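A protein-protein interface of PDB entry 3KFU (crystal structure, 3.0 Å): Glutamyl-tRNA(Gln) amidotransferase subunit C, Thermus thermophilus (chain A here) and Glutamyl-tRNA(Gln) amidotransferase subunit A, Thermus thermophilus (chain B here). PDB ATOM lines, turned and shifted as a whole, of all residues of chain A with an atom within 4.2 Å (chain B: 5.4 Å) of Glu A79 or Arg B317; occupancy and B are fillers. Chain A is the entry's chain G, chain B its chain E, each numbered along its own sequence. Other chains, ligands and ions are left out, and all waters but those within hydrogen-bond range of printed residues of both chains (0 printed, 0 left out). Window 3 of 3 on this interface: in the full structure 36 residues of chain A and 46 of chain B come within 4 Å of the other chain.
O of Leu B313 sits close to N of Ala A77, 3.4 Å away. NH2 of Arg B317 sits at hydrogen-bond distance from O of Arg A86, 2.8 Å away.
NH1 of Arg B317 lies within hydrogen-bond range of O of Gly B311 (3.1 Å). O of Thr B312 is in hydrogen-bond range of NH1 of Arg B317, at 3.4 Å. NE of Arg B317 sits close to SD of Met B326, 3.8 Å away. OG1 of Thr B330 sits at hydrogen-bond distance from O of Met B326 (3.1 Å). The backbone NH (N) of Arg A86 sits at hydrogen-bond distance from the backbone carbonyl oxygen (O) of Glu A79 (2.8 Å).
Pro A78 touches Gly B311. O of Thr B312 touches CD of Pro A78 (3.7 Å). Pro A78 touches Gly B315. Pro A78 touches Arg B317 (CB to NH1, 3.0 Å). NH1 of Arg B317 touches N of Glu A79 (3.7 Å). Leu B313 touches Phe A85. O of Thr B312 touches CG1 of Val A87, 3.9 Å away. Val A87 touches Arg B317. NH2 of Arg B317 touches CD of Pro A88 (3.4 Å). Pro A88 touches Met B326.
Printed residues of chain B within 4 Å of Glu A79: Arg B317 (3.7 Å). Arg B317 touches five residues of chain A. Of the printed residues of chain B, Arg A86 touches Arg B317. Of the printed residues of chain B, Pro A88 touches Arg B317 (3.4 Å) and Met B326 (3.6 Å). Of the printed residues of chain B, Val A87 touches Thr B312 and Arg B317. Arg B316 touches none of the printed residues of chain A. The nearest printed residue of chain A that does not touch Arg B317 is Ala A77 (5.3 Å). The nearest printed residue of chain B that does not touch Ala A77 is Thr B312 (5.3 Å).
Of the 10 printed residues of chain B, 6 touch a printed residue of chain A. Printed residues of chain B that touch a printed residue of chain A: Gly B311, Thr B312, Leu B313, Gly B315, Arg B317 and Met B326. Hydrophobic or aromatic side chains of chain B that line the printed part of chain A: Met B326. Along chain B the printed residues that touch a printed residue of chain A span positions 311 to 326. Of the 8 printed residues of chain A, 7 touch a printed residue of chain B. Hydrophobic or aromatic side chains of chain A that line the printed part of chain B: Ala A77, Pro A78, Phe A85, Val A87 and Pro A88. Among the printed residues, no Asp or Glu carboxylate lies within 4 Å of a Lys or Arg side-chain nitrogen of the other chain.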
ATOM      1  N   ALA A  77       4.631 -19.944  19.798  1.00  0.00           N
ATOM      2  CA  ALA A  77       5.144 -21.307  19.807  1.00  0.00           C
ATOM      3  C   ALA A  77       4.555 -22.128  20.937  1.00  0.00           C
ATOM      4  O   ALA A  77       4.495 -21.671  22.078  1.00  0.00           O
ATOM      5  CB  ALA A  77       6.659 -21.299  19.899  1.00  0.00           C
ATOM      6  N   PRO A  78       4.111 -23.350  20.620  1.00  0.00           N
ATOM      7  CA  PRO A  78       3.640 -24.284  21.644  1.00  0.00           C
ATOM      8  C   PRO A  78       4.792 -24.673  22.562  1.00  0.00           C
ATOM      9  O   PRO A  78       4.584 -24.933  23.747  1.00  0.00           O
ATOM     10  CB  PRO A  78       3.177 -25.494  20.827  1.00  0.00           C
ATOM     11  CG  PRO A  78       2.963 -24.965  19.432  1.00  0.00           C
ATOM     12  CD  PRO A  78       3.988 -23.903  19.261  1.00  0.00           C
ATOM     13  N   GLU A  79       5.999 -24.697  22.001  1.00  0.00           N
ATOM     14  CA  GLU A  79       7.214 -25.007  22.748  1.00  0.00           C
ATOM     15  C   GLU A  79       8.395 -24.185  22.242  1.00  0.00           C
ATOM     16  O   GLU A  79       8.674 -24.159  21.047  1.00  0.00           O
ATOM     17  CB  GLU A  79       7.555 -26.493  22.631  1.00  0.00           C
ATOM     18  CG  GLU A  79       6.880 -27.390  23.653  1.00  0.00           C
ATOM     19  CD  GLU A  79       7.405 -28.815  23.602  1.00  0.00           C
ATOM     20  OE1 GLU A  79       7.940 -29.221  22.548  1.00  0.00           O
ATOM     21  OE2 GLU A  79       7.288 -29.527  24.622  1.00  0.00           O
ATOM     22  N   ALA A  80       9.086 -23.519  23.161  1.00  0.00           N
ATOM     23  CA  ALA A  80      10.289 -22.762  22.827  1.00  0.00           C
ATOM     24  C   ALA A  80      11.415 -23.074  23.811  1.00  0.00           C
ATOM     25  O   ALA A  80      11.169 -23.503  24.938  1.00  0.00           O
ATOM     26  CB  ALA A  80       9.992 -21.274  22.811  1.00  0.00           C
ATOM     27  N   PHE A  85      12.244 -22.127  18.301  1.00  0.00           N
ATOM     28  CA  PHE A  85      11.018 -22.907  18.265  1.00  0.00           C
ATOM     29  C   PHE A  85      11.416 -24.358  18.483  1.00  0.00           C
ATOM     30  O   PHE A  85      12.327 -24.862  17.827  1.00  0.00           O
ATOM     31  CB  PHE A  85      10.298 -22.748  16.927  1.00  0.00           C
ATOM     32  CG  PHE A  85       9.701 -21.385  16.717  1.00  0.00           C
ATOM     33  CD1 PHE A  85       8.415 -21.104  17.146  1.00  0.00           C
ATOM     34  CD2 PHE A  85      10.423 -20.386  16.086  1.00  0.00           C
ATOM     35  CE1 PHE A  85       7.860 -19.851  16.954  1.00  0.00           C
ATOM     36  CE2 PHE A  85       9.875 -19.134  15.888  1.00  0.00           C
ATOM     37  CZ  PHE A  85       8.592 -18.865  16.324  1.00  0.00           C
ATOM     38  N   ARG A  86      10.746 -25.020  19.417  1.00  0.00           N
ATOM     39  CA  ARG A  86      11.092 -26.386  19.777  1.00  0.00           C
ATOM     40  C   ARG A  86      10.083 -27.393  19.243  1.00  0.00           C
ATOM     41  O   ARG A  86       8.893 -27.313  19.544  1.00  0.00           O
ATOM     42  CB  ARG A  86      11.201 -26.512  21.297  1.00  0.00           C
ATOM     43  CG  ARG A  86      11.563 -27.901  21.784  1.00  0.00           C
ATOM     44  CD  ARG A  86      11.775 -27.899  23.280  1.00  0.00           C
ATOM     45  NE  ARG A  86      12.139 -29.219  23.780  1.00  0.00           N
ATOM     46  CZ  ARG A  86      12.475 -29.465  25.041  1.00  0.00           C
ATOM     47  NH1 ARG A  86      12.493 -28.477  25.925  1.00  0.00           N
ATOM     48  NH2 ARG A  86      12.794 -30.696  25.416  1.00  0.00           N
ATOM     49  N   VAL A  87      10.563 -28.341  18.446  1.00  0.00           N
ATOM     50  CA  VAL A  87       9.713 -29.420  17.962  1.00  0.00           C
ATOM     51  C   VAL A  87      10.317 -30.786  18.282  1.00  0.00           C
ATOM     52  O   VAL A  87      11.527 -30.902  18.499  1.00  0.00           O
ATOM     53  CB  VAL A  87       9.476 -29.324  16.442  1.00  0.00           C
ATOM     54  CG1 VAL A  87       8.816 -27.998  16.085  1.00  0.00           C
ATOM     55  CG2 VAL A  87      10.782 -29.496  15.695  1.00  0.00           C
ATOM     56  N   PRO A  88       9.470 -31.826  18.326  1.00  0.00           N
ATOM     57  CA  PRO A  88       9.959 -33.199  18.457  1.00  0.00           C
ATOM     58  C   PRO A  88      11.034 -33.484  17.416  1.00  0.00           C
ATOM     59  O   PRO A  88      11.048 -32.846  16.363  1.00  0.00           O
ATOM     60  CB  PRO A  88       8.712 -34.031  18.174  1.00  0.00           C
ATOM     61  CG  PRO A  88       7.597 -33.177  18.659  1.00  0.00           C
ATOM     62  CD  PRO A  88       7.999 -31.760  18.349  1.00  0.00           C
ATOM     63  N   GLY B 311       1.489 -28.794  14.123  1.00  0.00           N
ATOM     64  CA  GLY B 311       1.661 -28.238  15.453  1.00  0.00           C
ATOM     65  C   GLY B 311       3.013 -27.603  15.724  1.00  0.00           C
ATOM     66  O   GLY B 311       3.349 -27.318  16.873  1.00  0.00           O
ATOM     67  N   THR B 312       3.790 -27.371  14.673  1.00  0.00           N
ATOM     68  CA  THR B 312       5.170 -26.911  14.837  1.00  0.00           C
ATOM     69  C   THR B 312       5.342 -25.534  15.488  1.00  0.00           C
ATOM     70  O   THR B 312       5.970 -25.420  16.541  1.00  0.00           O
ATOM     71  CB  THR B 312       5.953 -26.964  13.512  1.00  0.00           C
ATOM     72  OG1 THR B 312       5.256 -26.214  12.511  1.00  0.00           O
ATOM     73  CG2 THR B 312       6.118 -28.414  13.048  1.00  0.00           C
ATOM     74  N   LEU B 313       4.787 -24.492  14.879  1.00  0.00           N
ATOM     75  CA  LEU B 313       5.097 -23.130  15.320  1.00  0.00           C
ATOM     76  C   LEU B 313       3.981 -22.357  16.032  1.00  0.00           C
ATOM     77  O   LEU B 313       4.275 -21.449  16.807  1.00  0.00           O
ATOM     78  CB  LEU B 313       5.648 -22.292  14.164  1.00  0.00           C
ATOM     79  CG  LEU B 313       6.823 -22.917  13.415  1.00  0.00           C
ATOM     80  CD1 LEU B 313       6.342 -23.559  12.129  1.00  0.00           C
ATOM     81  CD2 LEU B 313       7.870 -21.871  13.117  1.00  0.00           C
ATOM     82  N   GLY B 315      -0.020 -23.577  15.931  1.00  0.00           N
ATOM     83  CA  GLY B 315      -1.308 -24.215  16.138  1.00  0.00           C
ATOM     84  C   GLY B 315      -1.430 -24.845  17.515  1.00  0.00           C
ATOM     85  O   GLY B 315      -0.661 -24.535  18.421  1.00  0.00           O
ATOM     86  N   ARG B 316      -2.414 -25.719  17.683  1.00  0.00           N
ATOM     87  CA  ARG B 316      -2.444 -26.602  18.839  1.00  0.00           C
ATOM     88  C   ARG B 316      -1.499 -27.753  18.542  1.00  0.00           C
ATOM     89  O   ARG B 316      -1.319 -28.122  17.384  1.00  0.00           O
ATOM     90  CB  ARG B 316      -3.844 -27.167  19.059  1.00  0.00           C
ATOM     91  CG  ARG B 316      -4.631 -26.504  20.167  1.00  0.00           C
ATOM     92  CD  ARG B 316      -5.893 -27.295  20.455  1.00  0.00           C
ATOM     93  NE  ARG B 316      -5.588 -28.683  20.789  1.00  0.00           N
ATOM     94  CZ  ARG B 316      -6.506 -29.621  21.002  1.00  0.00           C
ATOM     95  NH1 ARG B 316      -7.796 -29.324  20.906  1.00  0.00           N
ATOM     96  NH2 ARG B 316      -6.136 -30.858  21.303  1.00  0.00           N
ATOM     97  N   ARG B 317      -0.887 -28.312  19.579  1.00  0.00           N
ATOM     98  CA  ARG B 317      -0.109 -29.527  19.422  1.00  0.00           C
ATOM     99  C   ARG B 317      -0.971 -30.700  19.864  1.00  0.00           C
ATOM    100  O   ARG B 317      -1.581 -30.657  20.930  1.00  0.00           O
ATOM    101  CB  ARG B 317       1.173 -29.452  20.247  1.00  0.00           C
ATOM    102  CG  ARG B 317       2.442 -29.633  19.438  1.00  0.00           C
ATOM    103  CD  ARG B 317       3.670 -29.418  20.296  1.00  0.00           C
ATOM    104  NE  ARG B 317       4.911 -29.479  19.530  1.00  0.00           N
ATOM    105  CZ  ARG B 317       5.579 -28.415  19.099  1.00  0.00           C
ATOM    106  NH1 ARG B 317       5.127 -27.196  19.350  1.00  0.00           N
ATOM    107  NH2 ARG B 317       6.703 -28.570  18.415  1.00  0.00           N
ATOM    108  N   ALA B 318      -1.040 -31.737  19.034  1.00  0.00           N
ATOM    109  CA  ALA B 318      -1.900 -32.882  19.330  1.00  0.00           C
ATOM    110  C   ALA B 318      -1.208 -33.869  20.264  1.00  0.00           C
ATOM    111  O   ALA B 318      -1.837 -34.797  20.774  1.00  0.00           O
ATOM    112  CB  ALA B 318      -2.339 -33.578  18.053  1.00  0.00           C
ATOM    113  N   ALA B 319       0.044 -33.556  20.605  1.00  0.00           N
ATOM    114  CA  ALA B 319       0.872 -34.351  21.527  1.00  0.00           C
ATOM    115  C   ALA B 319       1.239 -35.794  21.142  1.00  0.00           C
ATOM    116  O   ALA B 319       1.186 -36.695  21.978  1.00  0.00           O
ATOM    117  CB  ALA B 319       0.260 -34.324  22.928  1.00  0.00           C
ATOM    118  N   MET B 326       3.216 -36.490  15.235  1.00  0.00           N
ATOM    119  CA  MET B 326       2.662 -35.275  15.818  1.00  0.00           C
ATOM    120  C   MET B 326       1.930 -34.450  14.764  1.00  0.00           C
ATOM    121  O   MET B 326       0.792 -34.035  14.971  1.00  0.00           O
ATOM    122  CB  MET B 326       3.765 -34.431  16.444  1.00  0.00           C
ATOM    123  CG  MET B 326       3.387 -32.967  16.586  1.00  0.00           C
ATOM    124  SD  MET B 326       4.829 -31.893  16.649  1.00  0.00           S
ATOM    125  CE  MET B 326       4.049 -30.296  16.644  1.00  0.00           C
ATOM    126  N   THR B 330      -2.004 -33.820  14.899  1.00  0.00           N
ATOM    127  CA  THR B 330      -2.466 -32.446  15.059  1.00  0.00           C
ATOM    128  C   THR B 330      -3.479 -32.083  13.987  1.00  0.00           C
ATOM    129  O   THR B 330      -4.505 -31.468  14.273  1.00  0.00           O
ATOM    130  CB  THR B 330      -1.296 -31.444  15.012  1.00  0.00           C
ATOM    131  OG1 THR B 330      -0.538 -31.534  16.225  1.00  0.00           O
ATOM    132  CG2 THR B 330      -1.819 -30.024  14.857  1.00  0.00           C
